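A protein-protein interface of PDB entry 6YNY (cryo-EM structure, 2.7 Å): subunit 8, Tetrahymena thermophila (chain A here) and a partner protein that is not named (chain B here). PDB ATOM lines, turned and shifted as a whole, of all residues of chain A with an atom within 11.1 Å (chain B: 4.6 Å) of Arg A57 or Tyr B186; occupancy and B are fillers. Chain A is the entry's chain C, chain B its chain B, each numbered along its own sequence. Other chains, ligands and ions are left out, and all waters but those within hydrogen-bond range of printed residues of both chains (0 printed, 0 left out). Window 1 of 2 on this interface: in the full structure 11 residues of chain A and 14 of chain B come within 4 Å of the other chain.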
ATOM      1  N   TRP A  49     -22.134 -13.935  20.100  1.00  0.00           N
ATOM      2  CA  TRP A  49     -21.534 -12.679  19.669  1.00  0.00           C
ATOM      3  C   TRP A  49     -20.815 -11.946  20.798  1.00  0.00           C
ATOM      4  O   TRP A  49     -19.787 -11.308  20.541  1.00  0.00           O
ATOM      5  CB  TRP A  49     -22.586 -11.773  19.020  1.00  0.00           C
ATOM      6  CG  TRP A  49     -23.535 -11.066  19.938  1.00  0.00           C
ATOM      7  CD1 TRP A  49     -24.819 -11.425  20.223  1.00  0.00           C
ATOM      8  CD2 TRP A  49     -23.289  -9.861  20.667  1.00  0.00           C
ATOM      9  NE1 TRP A  49     -25.380 -10.529  21.088  1.00  0.00           N
ATOM     10  CE2 TRP A  49     -24.463  -9.558  21.378  1.00  0.00           C
ATOM     11  CE3 TRP A  49     -22.189  -9.011  20.793  1.00  0.00           C
ATOM     12  CZ2 TRP A  49     -24.565  -8.448  22.200  1.00  0.00           C
ATOM     13  CZ3 TRP A  49     -22.295  -7.916  21.609  1.00  0.00           C
ATOM     14  CH2 TRP A  49     -23.473  -7.640  22.302  1.00  0.00           C
ATOM     15  N   PRO A  50     -21.292 -11.993  22.045  1.00  0.00           N
ATOM     16  CA  PRO A  50     -20.548 -11.291  23.099  1.00  0.00           C
ATOM     17  C   PRO A  50     -19.153 -11.851  23.300  1.00  0.00           C
ATOM     18  O   PRO A  50     -18.196 -11.091  23.473  1.00  0.00           O
ATOM     19  CB  PRO A  50     -21.435 -11.473  24.337  1.00  0.00           C
ATOM     20  CG  PRO A  50     -22.744 -11.904  23.824  1.00  0.00           C
ATOM     21  CD  PRO A  50     -22.463 -12.682  22.606  1.00  0.00           C
ATOM     22  N   THR A  51     -19.017 -13.175  23.270  1.00  0.00           N
ATOM     23  CA  THR A  51     -17.700 -13.796  23.360  1.00  0.00           C
ATOM     24  C   THR A  51     -16.837 -13.431  22.162  1.00  0.00           C
ATOM     25  O   THR A  51     -15.661 -13.085  22.309  1.00  0.00           O
ATOM     26  CB  THR A  51     -17.857 -15.311  23.463  1.00  0.00           C
ATOM     27  OG1 THR A  51     -18.501 -15.650  24.694  1.00  0.00           O
ATOM     28  CG2 THR A  51     -16.517 -15.994  23.383  1.00  0.00           C
ATOM     29  N   HIS A  52     -17.407 -13.508  20.961  1.00  0.00           N
ATOM     30  CA  HIS A  52     -16.651 -13.184  19.760  1.00  0.00           C
ATOM     31  C   HIS A  52     -16.264 -11.713  19.732  1.00  0.00           C
ATOM     32  O   HIS A  52     -15.145 -11.365  19.340  1.00  0.00           O
ATOM     33  CB  HIS A  52     -17.473 -13.545  18.529  1.00  0.00           C
ATOM     34  CG  HIS A  52     -16.788 -13.254  17.235  1.00  0.00           C
ATOM     35  ND1 HIS A  52     -17.164 -12.217  16.412  1.00  0.00           N
ATOM     36  CD2 HIS A  52     -15.751 -13.868  16.620  1.00  0.00           C
ATOM     37  CE1 HIS A  52     -16.389 -12.203  15.344  1.00  0.00           C
ATOM     38  NE2 HIS A  52     -15.523 -13.195  15.446  1.00  0.00           N
ATOM     39  N   PHE A  53     -17.179 -10.835  20.141  1.00  0.00           N
ATOM     40  CA  PHE A  53     -16.883  -9.410  20.150  1.00  0.00           C
ATOM     41  C   PHE A  53     -15.783  -9.080  21.147  1.00  0.00           C
ATOM     42  O   PHE A  53     -14.966  -8.189  20.898  1.00  0.00           O
ATOM     43  CB  PHE A  53     -18.154  -8.627  20.469  1.00  0.00           C
ATOM     44  CG  PHE A  53     -17.969  -7.146  20.471  1.00  0.00           C
ATOM     45  CD1 PHE A  53     -17.837  -6.451  19.287  1.00  0.00           C
ATOM     46  CD2 PHE A  53     -17.947  -6.442  21.657  1.00  0.00           C
ATOM     47  CE1 PHE A  53     -17.671  -5.091  19.288  1.00  0.00           C
ATOM     48  CE2 PHE A  53     -17.783  -5.080  21.660  1.00  0.00           C
ATOM     49  CZ  PHE A  53     -17.645  -4.403  20.473  1.00  0.00           C
ATOM     50  N   PHE A  54     -15.743  -9.790  22.272  1.00  0.00           N
ATOM     51  CA  PHE A  54     -14.757  -9.517  23.308  1.00  0.00           C
ATOM     52  C   PHE A  54     -13.389 -10.084  22.948  1.00  0.00           C
ATOM     53  O   PHE A  54     -12.376  -9.385  23.043  1.00  0.00           O
ATOM     54  CB  PHE A  54     -15.237 -10.094  24.637  1.00  0.00           C
ATOM     55  CG  PHE A  54     -14.285  -9.881  25.768  1.00  0.00           C
ATOM     56  CD1 PHE A  54     -14.285  -8.698  26.469  1.00  0.00           C
ATOM     57  CD2 PHE A  54     -13.391 -10.866  26.133  1.00  0.00           C
ATOM     58  CE1 PHE A  54     -13.416  -8.498  27.505  1.00  0.00           C
ATOM     59  CE2 PHE A  54     -12.522 -10.670  27.167  1.00  0.00           C
ATOM     60  CZ  PHE A  54     -12.532  -9.484  27.856  1.00  0.00           C
ATOM     61  N   ASN A  55     -13.340 -11.351  22.537  1.00  0.00           N
ATOM     62  CA  ASN A  55     -12.056 -11.999  22.294  1.00  0.00           C
ATOM     63  C   ASN A  55     -11.295 -11.323  21.164  1.00  0.00           C
ATOM     64  O   ASN A  55     -10.074 -11.148  21.248  1.00  0.00           O
ATOM     65  CB  ASN A  55     -12.270 -13.479  21.987  1.00  0.00           C
ATOM     66  CG  ASN A  55     -12.755 -14.258  23.187  1.00  0.00           C
ATOM     67  OD1 ASN A  55     -12.641 -13.809  24.324  1.00  0.00           O
ATOM     68  ND2 ASN A  55     -13.291 -15.439  22.939  1.00  0.00           N
ATOM     69  N   ARG A  56     -11.990 -10.940  20.099  1.00  0.00           N
ATOM     70  CA  ARG A  56     -11.343 -10.292  18.968  1.00  0.00           C
ATOM     71  C   ARG A  56     -10.838  -8.895  19.295  1.00  0.00           C
ATOM     72  O   ARG A  56     -10.218  -8.267  18.431  1.00  0.00           O
ATOM     73  CB  ARG A  56     -12.310 -10.220  17.788  1.00  0.00           C
ATOM     74  CG  ARG A  56     -12.840 -11.559  17.333  1.00  0.00           C
ATOM     75  CD  ARG A  56     -11.820 -12.372  16.565  1.00  0.00           C
ATOM     76  NE  ARG A  56     -11.641 -11.896  15.196  1.00  0.00           N
ATOM     77  CZ  ARG A  56     -10.694 -11.051  14.801  1.00  0.00           C
ATOM     78  NH1 ARG A  56     -10.628 -10.691  13.530  1.00  0.00           N
ATOM     79  NH2 ARG A  56      -9.813 -10.565  15.663  1.00  0.00           N
ATOM     80  N   ARG A  57     -11.081  -8.397  20.508  1.00  0.00           N
ATOM     81  CA  ARG A  57     -10.685  -7.053  20.892  1.00  0.00           C
ATOM     82  C   ARG A  57      -9.896  -6.984  22.190  1.00  0.00           C
ATOM     83  O   ARG A  57      -9.356  -5.918  22.497  1.00  0.00           O
ATOM     84  CB  ARG A  57     -11.924  -6.155  21.019  1.00  0.00           C
ATOM     85  CG  ARG A  57     -12.561  -5.831  19.688  1.00  0.00           C
ATOM     86  CD  ARG A  57     -13.965  -5.279  19.825  1.00  0.00           C
ATOM     87  NE  ARG A  57     -14.028  -4.129  20.719  1.00  0.00           N
ATOM     88  CZ  ARG A  57     -14.436  -4.170  21.982  1.00  0.00           C
ATOM     89  NH1 ARG A  57     -14.828  -5.308  22.534  1.00  0.00           N
ATOM     90  NH2 ARG A  57     -14.451  -3.060  22.698  1.00  0.00           N
ATOM     91  N   HIS A  58      -9.812  -8.071  22.956  1.00  0.00           N
ATOM     92  CA  HIS A  58      -9.109  -8.053  24.231  1.00  0.00           C
ATOM     93  C   HIS A  58      -8.204  -9.251  24.466  1.00  0.00           C
ATOM     94  O   HIS A  58      -7.488  -9.258  25.470  1.00  0.00           O
ATOM     95  CB  HIS A  58     -10.114  -7.972  25.385  1.00  0.00           C
ATOM     96  CG  HIS A  58     -10.983  -6.756  25.352  1.00  0.00           C
ATOM     97  ND1 HIS A  58     -10.642  -5.583  25.985  1.00  0.00           N
ATOM     98  CD2 HIS A  58     -12.184  -6.534  24.770  1.00  0.00           C
ATOM     99  CE1 HIS A  58     -11.593  -4.689  25.789  1.00  0.00           C
ATOM    100  NE2 HIS A  58     -12.540  -5.241  25.055  1.00  0.00           N
ATOM    101  N   SER A  59      -8.199 -10.253  23.593  1.00  0.00           N
ATOM    102  CA  SER A  59      -7.449 -11.480  23.816  1.00  0.00           C
ATOM    103  C   SER A  59      -6.006 -11.403  23.340  1.00  0.00           C
ATOM    104  O   SER A  59      -5.260 -12.370  23.523  1.00  0.00           O
ATOM    105  CB  SER A  59      -8.147 -12.653  23.126  1.00  0.00           C
ATOM    106  OG  SER A  59      -8.118 -12.518  21.717  1.00  0.00           O
ATOM    107  N   SER A  60      -5.593 -10.294  22.741  1.00  0.00           N
ATOM    108  CA  SER A  60      -4.231 -10.171  22.249  1.00  0.00           C
ATOM    109  C   SER A  60      -3.276  -9.832  23.384  1.00  0.00           C
ATOM    110  O   SER A  60      -3.643  -9.185  24.367  1.00  0.00           O
ATOM    111  CB  SER A  60      -4.145  -9.098  21.166  1.00  0.00           C
ATOM    112  OG  SER A  60      -4.467  -7.822  21.685  1.00  0.00           O
ATOM    113  N   SER A  61      -2.035 -10.286  23.236  1.00  0.00           N
ATOM    114  CA  SER A  61      -0.985 -10.029  24.207  1.00  0.00           C
ATOM    115  C   SER A  61       0.313  -9.736  23.471  1.00  0.00           C
ATOM    116  O   SER A  61       0.535 -10.215  22.358  1.00  0.00           O
ATOM    117  CB  SER A  61      -0.799 -11.213  25.157  1.00  0.00           C
ATOM    118  OG  SER A  61       0.072 -10.886  26.220  1.00  0.00           O
ATOM    119  N   GLN A  62       1.174  -8.945  24.112  1.00  0.00           N
ATOM    120  CA  GLN A  62       2.417  -8.518  23.482  1.00  0.00           C
ATOM    121  C   GLN A  62       3.471  -9.612  23.440  1.00  0.00           C
ATOM    122  O   GLN A  62       4.397  -9.523  22.627  1.00  0.00           O
ATOM    123  CB  GLN A  62       2.980  -7.295  24.208  1.00  0.00           C
ATOM    124  CG  GLN A  62       2.515  -5.976  23.628  1.00  0.00           C
ATOM    125  CD  GLN A  62       2.974  -5.786  22.193  1.00  0.00           C
ATOM    126  OE1 GLN A  62       4.173  -5.750  21.914  1.00  0.00           O
ATOM    127  NE2 GLN A  62       2.023  -5.686  21.276  1.00  0.00           N
ATOM    128  N   ARG A  66      -0.005 -11.664  16.906  1.00  0.00           N
ATOM    129  CA  ARG A  66      -1.378 -11.643  16.423  1.00  0.00           C
ATOM    130  C   ARG A  66      -1.351 -11.757  14.906  1.00  0.00           C
ATOM    131  O   ARG A  66      -0.804 -10.885  14.223  1.00  0.00           O
ATOM    132  CB  ARG A  66      -2.103 -10.371  16.858  1.00  0.00           C
ATOM    133  CG  ARG A  66      -3.544 -10.311  16.391  1.00  0.00           C
ATOM    134  CD  ARG A  66      -4.205  -8.997  16.728  1.00  0.00           C
ATOM    135  NE  ARG A  66      -5.454  -8.828  15.994  1.00  0.00           N
ATOM    136  CZ  ARG A  66      -6.116  -7.681  15.890  1.00  0.00           C
ATOM    137  NH1 ARG A  66      -5.653  -6.586  16.470  1.00  0.00           N
ATOM    138  NH2 ARG A  66      -7.240  -7.628  15.196  1.00  0.00           N
ATOM    139  N   PHE A  67      -1.933 -12.829  14.383  1.00  0.00           N
ATOM    140  CA  PHE A  67      -1.930 -13.082  12.953  1.00  0.00           C
ATOM    141  C   PHE A  67      -3.192 -12.531  12.311  1.00  0.00           C
ATOM    142  O   PHE A  67      -4.279 -12.585  12.889  1.00  0.00           O
ATOM    143  CB  PHE A  67      -1.804 -14.577  12.672  1.00  0.00           C
ATOM    144  CG  PHE A  67      -0.490 -15.158  13.087  1.00  0.00           C
ATOM    145  CD1 PHE A  67       0.619 -15.035  12.275  1.00  0.00           C
ATOM    146  CD2 PHE A  67      -0.360 -15.823  14.288  1.00  0.00           C
ATOM    147  CE1 PHE A  67       1.827 -15.564  12.654  1.00  0.00           C
ATOM    148  CE2 PHE A  67       0.848 -16.354  14.668  1.00  0.00           C
ATOM    149  CZ  PHE A  67       1.941 -16.223  13.850  1.00  0.00           C
ATOM    150  N   THR A  69      -6.393 -12.027   9.937  1.00  0.00           N
ATOM    151  CA  THR A  69      -7.443 -12.892   9.430  1.00  0.00           C
ATOM    152  C   THR A  69      -7.794 -12.517   7.993  1.00  0.00           C
ATOM    153  O   THR A  69      -7.230 -11.595   7.403  1.00  0.00           O
ATOM    154  CB  THR A  69      -8.686 -12.806  10.310  1.00  0.00           C
ATOM    155  OG1 THR A  69      -9.193 -11.467  10.296  1.00  0.00           O
ATOM    156  CG2 THR A  69      -8.359 -13.208  11.730  1.00  0.00           C
ATOM    157  N   GLU A  72      -9.360  -8.937   7.903  1.00  0.00           N
ATOM    158  CA  GLU A  72      -8.347  -7.913   8.105  1.00  0.00           C
ATOM    159  C   GLU A  72      -7.426  -7.769   6.901  1.00  0.00           C
ATOM    160  O   GLU A  72      -6.789  -6.724   6.746  1.00  0.00           O
ATOM    161  CB  GLU A  72      -7.543  -8.235   9.360  1.00  0.00           C
ATOM    162  CG  GLU A  72      -8.369  -8.205  10.633  1.00  0.00           C
ATOM    163  CD  GLU A  72      -7.668  -8.848  11.811  1.00  0.00           C
ATOM    164  OE1 GLU A  72      -6.604  -9.467  11.608  1.00  0.00           O
ATOM    165  OE2 GLU A  72      -8.184  -8.737  12.941  1.00  0.00           O
ATOM    166  N   MET B 182     -12.742  -3.734  31.435  1.00  0.00           N
ATOM    167  CA  MET B 182     -11.821  -3.933  30.323  1.00  0.00           C
ATOM    168  C   MET B 182     -12.284  -3.188  29.081  1.00  0.00           C
ATOM    169  O   MET B 182     -11.456  -2.706  28.301  1.00  0.00           O
ATOM    170  CB  MET B 182     -11.674  -5.419  30.022  1.00  0.00           C
ATOM    171  CG  MET B 182     -11.183  -6.232  31.194  1.00  0.00           C
ATOM    172  SD  MET B 182     -10.954  -7.969  30.803  1.00  0.00           S
ATOM    173  CE  MET B 182      -9.657  -7.847  29.579  1.00  0.00           C
ATOM    174  N   GLU B 183     -13.597  -3.095  28.874  1.00  0.00           N
ATOM    175  CA  GLU B 183     -14.116  -2.334  27.745  1.00  0.00           C
ATOM    176  C   GLU B 183     -13.902  -0.842  27.947  1.00  0.00           C
ATOM    177  O   GLU B 183     -13.616  -0.114  26.991  1.00  0.00           O
ATOM    178  CB  GLU B 183     -15.599  -2.639  27.546  1.00  0.00           C
ATOM    179  CG  GLU B 183     -15.895  -4.060  27.122  1.00  0.00           C
ATOM    180  CD  GLU B 183     -15.406  -4.364  25.720  1.00  0.00           C
ATOM    181  OE1 GLU B 183     -14.857  -3.451  25.072  1.00  0.00           O
ATOM    182  OE2 GLU B 183     -15.574  -5.514  25.265  1.00  0.00           O
ATOM    183  N   ALA B 184     -14.041  -0.369  29.185  1.00  0.00           N
ATOM    184  CA  ALA B 184     -13.816   1.041  29.464  1.00  0.00           C
ATOM    185  C   ALA B 184     -12.354   1.423  29.294  1.00  0.00           C
ATOM    186  O   ALA B 184     -12.050   2.586  29.008  1.00  0.00           O
ATOM    187  CB  ALA B 184     -14.287   1.373  30.876  1.00  0.00           C
ATOM    188  N   PHE B 185     -11.442   0.470  29.466  1.00  0.00           N
ATOM    189  CA  PHE B 185     -10.012   0.696  29.308  1.00  0.00           C
ATOM    190  C   PHE B 185      -9.474   0.097  28.014  1.00  0.00           C
ATOM    191  O   PHE B 185      -8.291  -0.234  27.922  1.00  0.00           O
ATOM    192  CB  PHE B 185      -9.258   0.133  30.508  1.00  0.00           C
ATOM    193  CG  PHE B 185      -9.425   0.939  31.756  1.00  0.00           C
ATOM    194  CD1 PHE B 185      -8.446   1.823  32.161  1.00  0.00           C
ATOM    195  CD2 PHE B 185     -10.562   0.817  32.525  1.00  0.00           C
ATOM    196  CE1 PHE B 185      -8.600   2.562  33.301  1.00  0.00           C
ATOM    197  CE2 PHE B 185     -10.718   1.557  33.665  1.00  0.00           C
ATOM    198  CZ  PHE B 185      -9.737   2.431  34.053  1.00  0.00           C
ATOM    199  N   TYR B 186     -10.330  -0.043  27.002  1.00  0.00           N
ATOM    200  CA  TYR B 186      -9.878  -0.593  25.731  1.00  0.00           C
ATOM    201  C   TYR B 186      -8.836   0.302  25.081  1.00  0.00           C
ATOM    202  O   TYR B 186      -7.812  -0.183  24.586  1.00  0.00           O
ATOM    203  CB  TYR B 186     -11.068  -0.787  24.796  1.00  0.00           C
ATOM    204  CG  TYR B 186     -10.682  -1.145  23.384  1.00  0.00           C
ATOM    205  CD1 TYR B 186     -10.239  -2.417  23.068  1.00  0.00           C
ATOM    206  CD2 TYR B 186     -10.765  -0.212  22.367  1.00  0.00           C
ATOM    207  CE1 TYR B 186      -9.885  -2.747  21.783  1.00  0.00           C
ATOM    208  CE2 TYR B 186     -10.413  -0.532  21.080  1.00  0.00           C
ATOM    209  CZ  TYR B 186      -9.973  -1.800  20.792  1.00  0.00           C
ATOM    210  OH  TYR B 186      -9.622  -2.123  19.507  1.00  0.00           O
ATOM    211  N   HIS B 187      -9.070   1.613  25.088  1.00  0.00           N
ATOM    212  CA  HIS B 187      -8.170   2.527  24.396  1.00  0.00           C
ATOM    213  C   HIS B 187      -6.784   2.515  25.021  1.00  0.00           C
ATOM    214  O   HIS B 187      -5.773   2.552  24.311  1.00  0.00           O
ATOM    215  CB  HIS B 187      -8.741   3.942  24.418  1.00  0.00           C
ATOM    216  CG  HIS B 187     -10.195   4.015  24.083  1.00  0.00           C
ATOM    217  ND1 HIS B 187     -11.182   3.720  24.997  1.00  0.00           N
ATOM    218  CD2 HIS B 187     -10.831   4.352  22.938  1.00  0.00           C
ATOM    219  CE1 HIS B 187     -12.364   3.871  24.429  1.00  0.00           C
ATOM    220  NE2 HIS B 187     -12.179   4.255  23.180  1.00  0.00           N
ATOM    221  N   GLU B 188      -6.715   2.466  26.351  1.00  0.00           N
ATOM    222  CA  GLU B 188      -5.424   2.452  27.026  1.00  0.00           C
ATOM    223  C   GLU B 188      -4.708   1.123  26.834  1.00  0.00           C
ATOM    224  O   GLU B 188      -3.500   1.096  26.575  1.00  0.00           O
ATOM    225  CB  GLU B 188      -5.617   2.744  28.511  1.00  0.00           C
ATOM    226  CG  GLU B 188      -6.194   4.112  28.798  1.00  0.00           C
ATOM    227  CD  GLU B 188      -7.707   4.123  28.802  1.00  0.00           C
ATOM    228  OE1 GLU B 188      -8.313   3.210  28.203  1.00  0.00           O
ATOM    229  OE2 GLU B 188      -8.291   5.046  29.407  1.00  0.00           O
ATOM    230  N   ASN B 189      -5.431   0.011  26.960  1.00  0.00           N
ATOM    231  CA  ASN B 189      -4.801  -1.296  26.818  1.00  0.00           C
ATOM    232  C   ASN B 189      -4.221  -1.483  25.425  1.00  0.00           C
ATOM    233  O   ASN B 189      -3.111  -2.002  25.270  1.00  0.00           O
ATOM    234  CB  ASN B 189      -5.806  -2.403  27.132  1.00  0.00           C
ATOM    235  CG  ASN B 189      -6.182  -2.452  28.592  1.00  0.00           C
ATOM    236  OD1 ASN B 189      -5.412  -2.044  29.458  1.00  0.00           O
ATOM    237  ND2 ASN B 189      -7.374  -2.960  28.878  1.00  0.00           N
ATOM    238  N   ILE B 190      -4.957  -1.063  24.397  1.00  0.00           N
ATOM    239  CA  ILE B 190      -4.488  -1.243  23.029  1.00  0.00           C
ATOM    240  C   ILE B 190      -3.354  -0.276  22.721  1.00  0.00           C
ATOM    241  O   ILE B 190      -2.371  -0.643  22.070  1.00  0.00           O
ATOM    242  CB  ILE B 190      -5.659  -1.078  22.045  1.00  0.00           C
ATOM    243  CG1 ILE B 190      -5.240  -1.473  20.631  1.00  0.00           C
ATOM    244  CG2 ILE B 190      -6.152   0.344  22.044  1.00  0.00           C
ATOM    245  CD1 ILE B 190      -4.992  -2.932  20.461  1.00  0.00           C
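OE1 of Glu B183 lies within salt-bridge range of NH2 of Arg A57 (2.4 Å).
The side-chain carboxylate of Glu B183 lies within hydrogen-bond range of a ring nitrogen (NE2) of His A58 (2.9 Å).
The backbone carbonyl oxygen (O) of Phe A53 sits close to the guanidinium group (NH1) of Arg A57, at 3.3 Å.
The guanidinium group (NH1) of Arg A57 sits at hydrogen-bond distance from a ring nitrogen (NE2) of His A58 (3.4 Å).
Of the 9 printed residues of chain B, 3 touch a printed residue of chain A.
Printed residues of chain B that touch a printed residue of chain A: Met B182, Glu B183 and Tyr B186.
Hydrophobic or aromatic side chains of chain B within 4 Å of the printed part of chain A: Met B182 and Tyr B186.
Along chain B the printed residues that touch a printed residue of chain A span positions 182 to 186.
Hydrophobic or aromatic side chains of chain A that line the printed part of chain B: Phe A54 and His A58.
Among the printed residues, 7 pairs touch across the chains.
Among the printed residues, pairs that only touch across the chains: His A58 with Met B182 (3.2 Å), Arg A57 with Tyr B186 (3.3 Å), Phe A54 with Glu B183 (3.6 Å), Phe A54 with Met B182 (3.7 Å) and His A58 with Tyr B186 (3.8 Å).
Arg A57 touches just these residues of chain B: Glu B183 (2.4 Å) and Tyr B186 (3.3 Å).
Printed residues of chain A within 4 Å of Tyr B186: Arg A57 and His A58.
Glu B183 touches just these residues of chain A: Phe A54, Arg A57 and His A58.
No residue of chain A comes within 4 Å of Ala B184.
No residue of chain A comes within 4 Å of His B187.
No residue of chain A comes within 4 Å of Asn B189.
Ile B190 touches none of the printed residues of chain A.
Of the printed residues of chain A, Met B182 touches Phe A54 and His A58.
Of the printed residues of chain B, His A58 touches Met B182, Glu B183 and Tyr B186.
Of the printed residues of chain B, Phe A54 touches Met B182 (3.7 Å) and Glu B183 (3.6 Å).
The nearest printed residue of chain B that does not touch Arg A57 is Ile B190 (5.7 Å).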
